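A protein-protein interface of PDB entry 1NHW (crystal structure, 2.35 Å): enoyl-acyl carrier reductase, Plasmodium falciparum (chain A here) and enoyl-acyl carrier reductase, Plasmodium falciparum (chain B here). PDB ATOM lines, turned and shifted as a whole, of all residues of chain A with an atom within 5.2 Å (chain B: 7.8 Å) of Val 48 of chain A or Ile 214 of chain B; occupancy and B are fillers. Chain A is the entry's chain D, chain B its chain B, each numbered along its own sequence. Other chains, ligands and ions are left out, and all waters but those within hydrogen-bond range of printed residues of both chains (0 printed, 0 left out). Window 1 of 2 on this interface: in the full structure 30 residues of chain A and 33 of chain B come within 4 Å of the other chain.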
ATOM      1  N   LEU A  21     -37.574  -5.242  25.780  1.00  0.00           N
ATOM      2  CA  LEU A  21     -36.632  -6.301  26.120  1.00  0.00           C
ATOM      3  C   LEU A  21     -35.757  -5.802  27.265  1.00  0.00           C
ATOM      4  O   LEU A  21     -35.036  -4.814  27.127  1.00  0.00           O
ATOM      5  CB  LEU A  21     -35.761  -6.661  24.911  1.00  0.00           C
ATOM      6  CG  LEU A  21     -34.751  -7.789  25.146  1.00  0.00           C
ATOM      7  CD1 LEU A  21     -35.492  -9.106  25.389  1.00  0.00           C
ATOM      8  CD2 LEU A  21     -33.833  -7.905  23.946  1.00  0.00           C
ATOM      9  N   ASP A  25     -34.397 -10.206  31.089  1.00  0.00           N
ATOM     10  CA  ASP A  25     -35.007 -11.192  30.207  1.00  0.00           C
ATOM     11  C   ASP A  25     -33.899 -12.131  29.745  1.00  0.00           C
ATOM     12  O   ASP A  25     -34.102 -13.339  29.643  1.00  0.00           O
ATOM     13  CB  ASP A  25     -35.677 -10.533  28.996  1.00  0.00           C
ATOM     14  CG  ASP A  25     -36.997  -9.858  29.349  1.00  0.00           C
ATOM     15  OD1 ASP A  25     -37.708 -10.361  30.241  1.00  0.00           O
ATOM     16  OD2 ASP A  25     -37.338  -8.832  28.726  1.00  0.00           O
ATOM     17  N   ILE A  26     -32.729 -11.564  29.465  1.00  0.00           N
ATOM     18  CA  ILE A  26     -31.565 -12.335  29.052  1.00  0.00           C
ATOM     19  C   ILE A  26     -31.017 -13.000  30.311  1.00  0.00           C
ATOM     20  O   ILE A  26     -30.551 -14.149  30.277  1.00  0.00           O
ATOM     21  CB  ILE A  26     -30.462 -11.423  28.433  1.00  0.00           C
ATOM     22  CG1 ILE A  26     -30.713 -11.232  26.933  1.00  0.00           C
ATOM     23  CG2 ILE A  26     -29.071 -12.017  28.674  1.00  0.00           C
ATOM     24  CD1 ILE A  26     -32.021 -10.536  26.595  1.00  0.00           C
ATOM     25  N   VAL A  29     -32.636 -16.372  31.218  1.00  0.00           N
ATOM     26  CA  VAL A  29     -32.264 -17.378  30.235  1.00  0.00           C
ATOM     27  C   VAL A  29     -30.820 -17.796  30.511  1.00  0.00           C
ATOM     28  O   VAL A  29     -30.492 -18.979  30.448  1.00  0.00           O
ATOM     29  CB  VAL A  29     -32.388 -16.826  28.800  1.00  0.00           C
ATOM     30  CG1 VAL A  29     -31.952 -17.881  27.790  1.00  0.00           C
ATOM     31  CG2 VAL A  29     -33.822 -16.409  28.538  1.00  0.00           C
ATOM     32  N   ALA A  30     -29.965 -16.823  30.826  1.00  0.00           N
ATOM     33  CA  ALA A  30     -28.561 -17.098  31.138  1.00  0.00           C
ATOM     34  C   ALA A  30     -28.523 -17.990  32.361  1.00  0.00           C
ATOM     35  O   ALA A  30     -27.788 -18.965  32.420  1.00  0.00           O
ATOM     36  CB  ALA A  30     -27.816 -15.800  31.428  1.00  0.00           C
ATOM     37  N   LEU A  33     -29.272 -21.522  31.424  1.00  0.00           N
ATOM     38  CA  LEU A  33     -28.170 -22.147  30.700  1.00  0.00           C
ATOM     39  C   LEU A  33     -26.983 -22.471  31.602  1.00  0.00           C
ATOM     40  O   LEU A  33     -26.200 -23.371  31.300  1.00  0.00           O
ATOM     41  CB  LEU A  33     -27.724 -21.256  29.535  1.00  0.00           C
ATOM     42  CG  LEU A  33     -28.671 -21.236  28.326  1.00  0.00           C
ATOM     43  CD1 LEU A  33     -28.269 -20.144  27.353  1.00  0.00           C
ATOM     44  CD2 LEU A  33     -28.644 -22.593  27.642  1.00  0.00           C
ATOM     45  N   ILE A  46     -28.335 -19.398  21.402  1.00  0.00           N
ATOM     46  CA  ILE A  46     -29.734 -19.251  21.784  1.00  0.00           C
ATOM     47  C   ILE A  46     -30.167 -17.797  21.611  1.00  0.00           C
ATOM     48  O   ILE A  46     -29.551 -16.875  22.159  1.00  0.00           O
ATOM     49  CB  ILE A  46     -29.960 -19.671  23.259  1.00  0.00           C
ATOM     50  CG1 ILE A  46     -29.384 -21.072  23.505  1.00  0.00           C
ATOM     51  CG2 ILE A  46     -31.461 -19.659  23.587  1.00  0.00           C
ATOM     52  CD1 ILE A  46     -30.167 -22.176  22.848  1.00  0.00           C
ATOM     53  N   TYR A  47     -31.233 -17.601  20.848  1.00  0.00           N
ATOM     54  CA  TYR A  47     -31.759 -16.267  20.587  1.00  0.00           C
ATOM     55  C   TYR A  47     -32.781 -15.837  21.623  1.00  0.00           C
ATOM     56  O   TYR A  47     -33.782 -16.521  21.844  1.00  0.00           O
ATOM     57  CB  TYR A  47     -32.405 -16.217  19.200  1.00  0.00           C
ATOM     58  CG  TYR A  47     -31.420 -16.054  18.072  1.00  0.00           C
ATOM     59  CD1 TYR A  47     -31.081 -14.789  17.598  1.00  0.00           C
ATOM     60  CD2 TYR A  47     -30.805 -17.167  17.488  1.00  0.00           C
ATOM     61  CE1 TYR A  47     -30.158 -14.634  16.572  1.00  0.00           C
ATOM     62  CE2 TYR A  47     -29.875 -17.018  16.459  1.00  0.00           C
ATOM     63  CZ  TYR A  47     -29.561 -15.746  16.008  1.00  0.00           C
ATOM     64  OH  TYR A  47     -28.651 -15.581  14.988  1.00  0.00           O
ATOM     65  N   VAL A  48     -32.512 -14.699  22.255  1.00  0.00           N
ATOM     66  CA  VAL A  48     -33.402 -14.114  23.256  1.00  0.00           C
ATOM     67  C   VAL A  48     -33.599 -12.694  22.735  1.00  0.00           C
ATOM     68  O   VAL A  48     -32.920 -11.757  23.152  1.00  0.00           O
ATOM     69  CB  VAL A  48     -32.740 -14.090  24.648  1.00  0.00           C
ATOM     70  CG1 VAL A  48     -33.712 -13.538  25.674  1.00  0.00           C
ATOM     71  CG2 VAL A  48     -32.312 -15.479  25.036  1.00  0.00           C
ATOM     72  N   ASP A  49     -34.534 -12.556  21.802  1.00  0.00           N
ATOM     73  CA  ASP A  49     -34.771 -11.281  21.145  1.00  0.00           C
ATOM     74  C   ASP A  49     -36.230 -11.094  20.758  1.00  0.00           C
ATOM     75  O   ASP A  49     -36.520 -10.522  19.709  1.00  0.00           O
ATOM     76  CB  ASP A  49     -33.920 -11.238  19.883  1.00  0.00           C
ATOM     77  CG  ASP A  49     -34.334 -12.304  18.872  1.00  0.00           C
ATOM     78  OD1 ASP A  49     -35.161 -13.172  19.231  1.00  0.00           O
ATOM     79  OD2 ASP A  49     -33.839 -12.279  17.722  1.00  0.00           O
ATOM     80  N   ASN A  50     -37.138 -11.564  21.607  1.00  0.00           N
ATOM     81  CA  ASN A  50     -38.571 -11.474  21.337  1.00  0.00           C
ATOM     82  C   ASN A  50     -38.901 -12.013  19.949  1.00  0.00           C
ATOM     83  O   ASN A  50     -39.918 -11.652  19.358  1.00  0.00           O
ATOM     84  CB  ASN A  50     -39.066 -10.035  21.467  1.00  0.00           C
ATOM     85  CG  ASN A  50     -39.040  -9.531  22.899  1.00  0.00           C
ATOM     86  OD1 ASN A  50     -39.247 -10.290  23.842  1.00  0.00           O
ATOM     87  ND2 ASN A  50     -38.808  -8.240  23.063  1.00  0.00           N
ATOM     88  N   TYR B  15     -26.056  -5.928  30.150  1.00  0.00           N
ATOM     89  CA  TYR B  15     -26.543  -7.296  30.309  1.00  0.00           C
ATOM     90  C   TYR B  15     -25.845  -8.015  31.457  1.00  0.00           C
ATOM     91  O   TYR B  15     -26.439  -8.869  32.120  1.00  0.00           O
ATOM     92  CB  TYR B  15     -26.350  -8.088  29.013  1.00  0.00           C
ATOM     93  CG  TYR B  15     -27.447  -7.869  28.001  1.00  0.00           C
ATOM     94  CD1 TYR B  15     -28.779  -8.070  28.343  1.00  0.00           C
ATOM     95  CD2 TYR B  15     -27.156  -7.487  26.694  1.00  0.00           C
ATOM     96  CE1 TYR B  15     -29.796  -7.898  27.415  1.00  0.00           C
ATOM     97  CE2 TYR B  15     -28.168  -7.312  25.754  1.00  0.00           C
ATOM     98  CZ  TYR B  15     -29.486  -7.521  26.124  1.00  0.00           C
ATOM     99  OH  TYR B  15     -30.497  -7.366  25.204  1.00  0.00           O
ATOM    100  N   ILE B  19     -27.855 -10.214  34.270  1.00  0.00           N
ATOM    101  CA  ILE B  19     -27.482 -11.599  34.497  1.00  0.00           C
ATOM    102  C   ILE B  19     -27.178 -11.772  35.980  1.00  0.00           C
ATOM    103  O   ILE B  19     -27.677 -12.701  36.617  1.00  0.00           O
ATOM    104  CB  ILE B  19     -26.244 -11.990  33.666  1.00  0.00           C
ATOM    105  CG1 ILE B  19     -26.620 -12.024  32.186  1.00  0.00           C
ATOM    106  CG2 ILE B  19     -25.710 -13.347  34.116  1.00  0.00           C
ATOM    107  CD1 ILE B  19     -25.431 -12.101  31.261  1.00  0.00           C
ATOM    108  N   HIS B 118     -19.088 -14.568  30.019  1.00  0.00           N
ATOM    109  CA  HIS B 118     -18.299 -13.670  29.187  1.00  0.00           C
ATOM    110  C   HIS B 118     -19.266 -12.584  28.703  1.00  0.00           C
ATOM    111  O   HIS B 118     -20.058 -12.799  27.783  1.00  0.00           O
ATOM    112  CB  HIS B 118     -17.702 -14.426  28.006  1.00  0.00           C
ATOM    113  CG  HIS B 118     -16.848 -13.576  27.118  1.00  0.00           C
ATOM    114  ND1 HIS B 118     -17.375 -12.705  26.189  1.00  0.00           N
ATOM    115  CD2 HIS B 118     -15.502 -13.455  27.026  1.00  0.00           C
ATOM    116  CE1 HIS B 118     -16.390 -12.086  25.563  1.00  0.00           C
ATOM    117  NE2 HIS B 118     -15.244 -12.523  26.051  1.00  0.00           N
ATOM    118  N   ILE B 166     -20.543 -22.379  30.863  1.00  0.00           N
ATOM    119  CA  ILE B 166     -20.009 -21.104  30.394  1.00  0.00           C
ATOM    120  C   ILE B 166     -20.905 -20.502  29.305  1.00  0.00           C
ATOM    121  O   ILE B 166     -21.393 -21.213  28.427  1.00  0.00           O
ATOM    122  CB  ILE B 166     -18.601 -21.310  29.799  1.00  0.00           C
ATOM    123  CG1 ILE B 166     -17.685 -21.931  30.858  1.00  0.00           C
ATOM    124  CG2 ILE B 166     -18.049 -19.982  29.249  1.00  0.00           C
ATOM    125  CD1 ILE B 166     -16.282 -22.226  30.359  1.00  0.00           C
ATOM    126  N   ILE B 167     -21.131 -19.196  29.363  1.00  0.00           N
ATOM    127  CA  ILE B 167     -21.941 -18.541  28.343  1.00  0.00           C
ATOM    128  C   ILE B 167     -21.304 -17.222  27.944  1.00  0.00           C
ATOM    129  O   ILE B 167     -20.477 -16.673  28.668  1.00  0.00           O
ATOM    130  CB  ILE B 167     -23.379 -18.224  28.822  1.00  0.00           C
ATOM    131  CG1 ILE B 167     -23.321 -17.244  29.991  1.00  0.00           C
ATOM    132  CG2 ILE B 167     -24.121 -19.508  29.169  1.00  0.00           C
ATOM    133  CD1 ILE B 167     -24.612 -16.509  30.239  1.00  0.00           C
ATOM    134  N   SER B 168     -21.702 -16.720  26.783  1.00  0.00           N
ATOM    135  CA  SER B 168     -21.205 -15.448  26.284  1.00  0.00           C
ATOM    136  C   SER B 168     -22.388 -14.773  25.603  1.00  0.00           C
ATOM    137  O   SER B 168     -23.464 -15.361  25.491  1.00  0.00           O
ATOM    138  CB  SER B 168     -20.059 -15.661  25.295  1.00  0.00           C
ATOM    139  OG  SER B 168     -20.490 -16.408  24.169  1.00  0.00           O
ATOM    140  N   LEU B 169     -22.189 -13.541  25.158  1.00  0.00           N
ATOM    141  CA  LEU B 169     -23.240 -12.775  24.496  1.00  0.00           C
ATOM    142  C   LEU B 169     -22.869 -12.469  23.058  1.00  0.00           C
ATOM    143  O   LEU B 169     -21.790 -11.956  22.791  1.00  0.00           O
ATOM    144  CB  LEU B 169     -23.464 -11.438  25.215  1.00  0.00           C
ATOM    145  CG  LEU B 169     -24.261 -11.331  26.515  1.00  0.00           C
ATOM    146  CD1 LEU B 169     -25.657 -11.855  26.254  1.00  0.00           C
ATOM    147  CD2 LEU B 169     -23.592 -12.101  27.634  1.00  0.00           C
ATOM    148  N   THR B 170     -23.764 -12.771  22.130  1.00  0.00           N
ATOM    149  CA  THR B 170     -23.500 -12.461  20.732  1.00  0.00           C
ATOM    150  C   THR B 170     -24.656 -11.625  20.165  1.00  0.00           C
ATOM    151  O   THR B 170     -25.620 -11.329  20.872  1.00  0.00           O
ATOM    152  CB  THR B 170     -23.308 -13.742  19.898  1.00  0.00           C
ATOM    153  OG1 THR B 170     -22.859 -13.384  18.587  1.00  0.00           O
ATOM    154  CG2 THR B 170     -24.610 -14.517  19.797  1.00  0.00           C
ATOM    155  N   TYR B 171     -24.549 -11.239  18.898  1.00  0.00           N
ATOM    156  CA  TYR B 171     -25.580 -10.433  18.249  1.00  0.00           C
ATOM    157  C   TYR B 171     -25.812 -10.986  16.844  1.00  0.00           C
ATOM    158  O   TYR B 171     -24.901 -11.552  16.236  1.00  0.00           O
ATOM    159  CB  TYR B 171     -25.141  -8.967  18.188  1.00  0.00           C
ATOM    160  CG  TYR B 171     -26.182  -8.035  17.613  1.00  0.00           C
ATOM    161  CD1 TYR B 171     -27.474  -7.988  18.142  1.00  0.00           C
ATOM    162  CD2 TYR B 171     -25.880  -7.205  16.532  1.00  0.00           C
ATOM    163  CE1 TYR B 171     -28.443  -7.143  17.611  1.00  0.00           C
ATOM    164  CE2 TYR B 171     -26.842  -6.348  15.985  1.00  0.00           C
ATOM    165  CZ  TYR B 171     -28.125  -6.323  16.530  1.00  0.00           C
ATOM    166  OH  TYR B 171     -29.090  -5.487  15.989  1.00  0.00           O
ATOM    167  N   HIS B 172     -27.034 -10.820  16.340  1.00  0.00           N
ATOM    168  CA  HIS B 172     -27.420 -11.331  15.026  1.00  0.00           C
ATOM    169  C   HIS B 172     -26.634 -10.743  13.848  1.00  0.00           C
ATOM    170  O   HIS B 172     -26.624 -11.316  12.761  1.00  0.00           O
ATOM    171  CB  HIS B 172     -28.924 -11.108  14.823  1.00  0.00           C
ATOM    172  CG  HIS B 172     -29.526 -11.958  13.747  1.00  0.00           C
ATOM    173  ND1 HIS B 172     -29.288 -13.312  13.647  1.00  0.00           N
ATOM    174  CD2 HIS B 172     -30.406 -11.657  12.761  1.00  0.00           C
ATOM    175  CE1 HIS B 172     -29.998 -13.810  12.650  1.00  0.00           C
ATOM    176  NE2 HIS B 172     -30.687 -12.827  12.097  1.00  0.00           N
ATOM    177  N   LYS B 189     -18.269 -11.345  16.346  1.00  0.00           N
ATOM    178  CA  LYS B 189     -19.391 -12.184  16.757  1.00  0.00           C
ATOM    179  C   LYS B 189     -19.488 -13.479  15.948  1.00  0.00           C
ATOM    180  O   LYS B 189     -19.825 -14.537  16.493  1.00  0.00           O
ATOM    181  CB  LYS B 189     -20.702 -11.402  16.643  1.00  0.00           C
ATOM    182  CG  LYS B 189     -20.768 -10.222  17.595  1.00  0.00           C
ATOM    183  CD  LYS B 189     -20.453 -10.655  19.028  1.00  0.00           C
ATOM    184  CE  LYS B 189     -20.552  -9.483  19.999  1.00  0.00           C
ATOM    185  NZ  LYS B 189     -20.299  -9.882  21.411  1.00  0.00           N
ATOM    186  N   LEU B 192     -16.817 -15.633  17.442  1.00  0.00           N
ATOM    187  CA  LEU B 192     -17.232 -16.073  18.769  1.00  0.00           C
ATOM    188  C   LEU B 192     -18.251 -17.219  18.713  1.00  0.00           C
ATOM    189  O   LEU B 192     -18.163 -18.184  19.475  1.00  0.00           O
ATOM    190  CB  LEU B 192     -17.835 -14.888  19.529  1.00  0.00           C
ATOM    191  CG  LEU B 192     -18.331 -15.092  20.963  1.00  0.00           C
ATOM    192  CD1 LEU B 192     -17.260 -14.649  21.949  1.00  0.00           C
ATOM    193  CD2 LEU B 192     -19.586 -14.264  21.184  1.00  0.00           C
ATOM    194  N   GLU B 193     -19.217 -17.099  17.814  1.00  0.00           N
ATOM    195  CA  GLU B 193     -20.260 -18.102  17.662  1.00  0.00           C
ATOM    196  C   GLU B 193     -19.704 -19.405  17.134  1.00  0.00           C
ATOM    197  O   GLU B 193     -20.149 -20.480  17.520  1.00  0.00           O
ATOM    198  CB  GLU B 193     -21.349 -17.584  16.716  1.00  0.00           C
ATOM    199  CG  GLU B 193     -22.380 -16.704  17.393  1.00  0.00           C
ATOM    200  CD  GLU B 193     -23.405 -16.142  16.427  1.00  0.00           C
ATOM    201  OE1 GLU B 193     -23.820 -16.880  15.516  1.00  0.00           O
ATOM    202  OE2 GLU B 193     -23.807 -14.972  16.580  1.00  0.00           O
ATOM    203  N   THR B 196     -17.626 -21.014  19.846  1.00  0.00           N
ATOM    204  CA  THR B 196     -18.434 -21.598  20.904  1.00  0.00           C
ATOM    205  C   THR B 196     -18.626 -23.073  20.595  1.00  0.00           C
ATOM    206  O   THR B 196     -18.533 -23.915  21.487  1.00  0.00           O
ATOM    207  CB  THR B 196     -19.811 -20.900  21.021  1.00  0.00           C
ATOM    208  OG1 THR B 196     -19.627 -19.554  21.476  1.00  0.00           O
ATOM    209  CG2 THR B 196     -20.691 -21.618  22.021  1.00  0.00           C
ATOM    210  N   ASN B 212     -22.303 -22.216  25.849  1.00  0.00           N
ATOM    211  CA  ASN B 212     -23.330 -21.775  24.904  1.00  0.00           C
ATOM    212  C   ASN B 212     -23.225 -20.259  24.757  1.00  0.00           C
ATOM    213  O   ASN B 212     -22.526 -19.597  25.526  1.00  0.00           O
ATOM    214  CB  ASN B 212     -24.742 -22.127  25.413  1.00  0.00           C
ATOM    215  CG  ASN B 212     -25.019 -23.638  25.426  1.00  0.00           C
ATOM    216  OD1 ASN B 212     -25.224 -24.259  24.378  1.00  0.00           O
ATOM    217  ND2 ASN B 212     -25.030 -24.227  26.617  1.00  0.00           N
ATOM    218  N   THR B 213     -23.913 -19.706  23.766  1.00  0.00           N
ATOM    219  CA  THR B 213     -23.879 -18.267  23.577  1.00  0.00           C
ATOM    220  C   THR B 213     -25.290 -17.725  23.403  1.00  0.00           C
ATOM    221  O   THR B 213     -26.119 -18.327  22.715  1.00  0.00           O
ATOM    222  CB  THR B 213     -23.003 -17.876  22.367  1.00  0.00           C
ATOM    223  OG1 THR B 213     -22.859 -16.452  22.329  1.00  0.00           O
ATOM    224  CG2 THR B 213     -23.620 -18.352  21.071  1.00  0.00           C
ATOM    225  N   ILE B 214     -25.577 -16.608  24.064  1.00  0.00           N
ATOM    226  CA  ILE B 214     -26.894 -15.995  23.956  1.00  0.00           C
ATOM    227  C   ILE B 214     -26.853 -14.855  22.949  1.00  0.00           C
ATOM    228  O   ILE B 214     -26.029 -13.956  23.054  1.00  0.00           O
ATOM    229  CB  ILE B 214     -27.372 -15.423  25.314  1.00  0.00           C
ATOM    230  CG1 ILE B 214     -27.687 -16.562  26.283  1.00  0.00           C
ATOM    231  CG2 ILE B 214     -28.609 -14.545  25.114  1.00  0.00           C
ATOM    232  CD1 ILE B 214     -28.039 -16.080  27.674  1.00  0.00           C
ATOM    233  N   SER B 215     -27.741 -14.904  21.963  1.00  0.00           N
ATOM    234  CA  SER B 215     -27.818 -13.857  20.956  1.00  0.00           C
ATOM    235  C   SER B 215     -28.954 -12.950  21.410  1.00  0.00           C
ATOM    236  O   SER B 215     -30.134 -13.240  21.177  1.00  0.00           O
ATOM    237  CB  SER B 215     -28.123 -14.468  19.585  1.00  0.00           C
ATOM    238  OG  SER B 215     -27.937 -13.520  18.554  1.00  0.00           O
ATOM    239  N   ALA B 216     -28.594 -11.852  22.066  1.00  0.00           N
ATOM    240  CA  ALA B 216     -29.582 -10.916  22.598  1.00  0.00           C
ATOM    241  C   ALA B 216     -30.117  -9.841  21.645  1.00  0.00           C
ATOM    242  O   ALA B 216     -29.529  -9.539  20.605  1.00  0.00           O
ATOM    243  CB  ALA B 216     -29.018 -10.251  23.851  1.00  0.00           C
ATOM    244  N   GLY B 217     -31.256  -9.273  22.024  1.00  0.00           N
ATOM    245  CA  GLY B 217     -31.859  -8.214  21.237  1.00  0.00           C
ATOM    246  C   GLY B 217     -31.194  -6.901  21.624  1.00  0.00           C
ATOM    247  O   GLY B 217     -30.188  -6.916  22.333  1.00  0.00           O
ATOM    248  N   PRO B 218     -31.735  -5.751  21.195  1.00  0.00           N
ATOM    249  CA  PRO B 218     -31.174  -4.431  21.501  1.00  0.00           C
ATOM    250  C   PRO B 218     -31.432  -3.951  22.926  1.00  0.00           C
ATOM    251  O   PRO B 218     -32.556  -4.010  23.428  1.00  0.00           O
ATOM    252  CB  PRO B 218     -31.847  -3.510  20.482  1.00  0.00           C
ATOM    253  CG  PRO B 218     -32.488  -4.431  19.488  1.00  0.00           C
ATOM    254  CD  PRO B 218     -32.886  -5.619  20.293  1.00  0.00           C
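Val 48 of chain A touches four residues of chain B.
Of chain A, only Ala 30, Leu 33, Ile 46 and Val 48 come within 4 Å of Ile 214 of chain B.
Of the printed residues of chain B, Leu 21 of chain A touches Tyr 15 (3.6 Å) and Gly 217 (3.4 Å).
Of the printed residues of chain B, Asp 49 of chain A touches Gly 217 (3.9 Å).
Of the printed residues of chain B, Ala 30 of chain A touches Ile 167 and Ile 214.
Asn 212 of chain B touches none of the printed residues of chain A.
Ser 168 of chain B touches none of the printed residues of chain A.
The nearest printed residue of chain B that does not touch Leu 33 of chain A is Ile 167 of chain B (4.02 Å).
Hydrophobic or aromatic side chains of chain A within 4 Å of the printed part of chain B: Leu 21, Ile 26, Ala 30, Leu 33, Tyr 47 and Val 48.
Hydrophobic or aromatic side chains of chain B that line the printed part of chain A: Tyr 15, Ile 167, His 172, Ile 214 and Ala 216.
Along chain B the printed residues that touch a printed residue of chain A span positions 15 to 217.
Among the printed residues, 17 pairs touch across the chains.
Among the printed residues, no Asp or Glu carboxylate lies within 4 Å of a Lys or Arg side-chain nitrogen of the other chain.
The backbone carbonyl oxygen of Thr 170 of chain B is in hydrogen-bond range of the backbone NH of Ala 216 of chain B.
The backbone NH (N) of His 118 of chain B lies within hydrogen-bond range of the backbone carbonyl oxygen (O) of Ile 167 of chain B, at 2.9 Å.
The side-chain hydroxyl (OH) of Tyr 15 of chain B is in hydrogen-bond range of the backbone carbonyl oxygen (O) of Gly 217 of chain B (2.9 Å).
N of Thr 170 of chain B sits at hydrogen-bond distance from O of Ile 214 of chain B (2.7 Å).
The side-chain hydroxyl (OG1) of Thr 213 of chain B sits at hydrogen-bond distance from the side-chain hydroxyl (OG) of Ser 168 of chain B (3.0 Å).
The backbone NH (N) of Ile 214 of chain B sits at hydrogen-bond distance from the backbone carbonyl oxygen (O) of Ser 168 of chain B, at 2.8 Å.
Among the printed residues, pairs that only touch across the chains: Tyr 47 of chain A with Ser 215 of chain B (3.2 Å), Ile 46 of chain A with Ile 214 of chain B (3.3 Å), Leu 21 of chain A with Gly 217 of chain B (3.4 Å), Val 48 of chain A with Ala 216 of chain B (3.5 Å), Ala 30 of chain A with Ile 167 of chain B (3.5 Å), Ile 26 of chain A with Tyr 15 of chain B (3.5 Å), Leu 21 of chain A with Tyr 15 of chain B (3.6 Å), Ala 30 of chain A with Ile 214 of chain B (3.6 Å), Ile 26 of chain A with Ala 216 of chain B (3.7 Å), Leu 33 of chain A with Ile 214 of chain B (3.8 Å), Val 48 of chain A with Ile 214 of chain B (3.8 Å) and Asp 49 of chain A with Gly 217 of chain B (3.9 Å).
N of Gly 217 of chain B is in hydrogen-bond range of O of Val 48 of chain A (3.2 Å).
N of Ile 46 of chain A lies within hydrogen-bond range of O of Thr 213 of chain B, 2.8 Å away.
The side-chain hydroxyl of Tyr 47 of chain A lies within hydrogen-bond range of a ring nitrogen (ND1) of His 172 of chain B (2.7 Å).
The backbone NH of Ser 215 of chain B lies within hydrogen-bond range of the backbone carbonyl oxygen of Ile 46 of chain A (2.7 Å).
O of Ser 215 of chain B lies within hydrogen-bond range of N of Val 48 of chain A.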
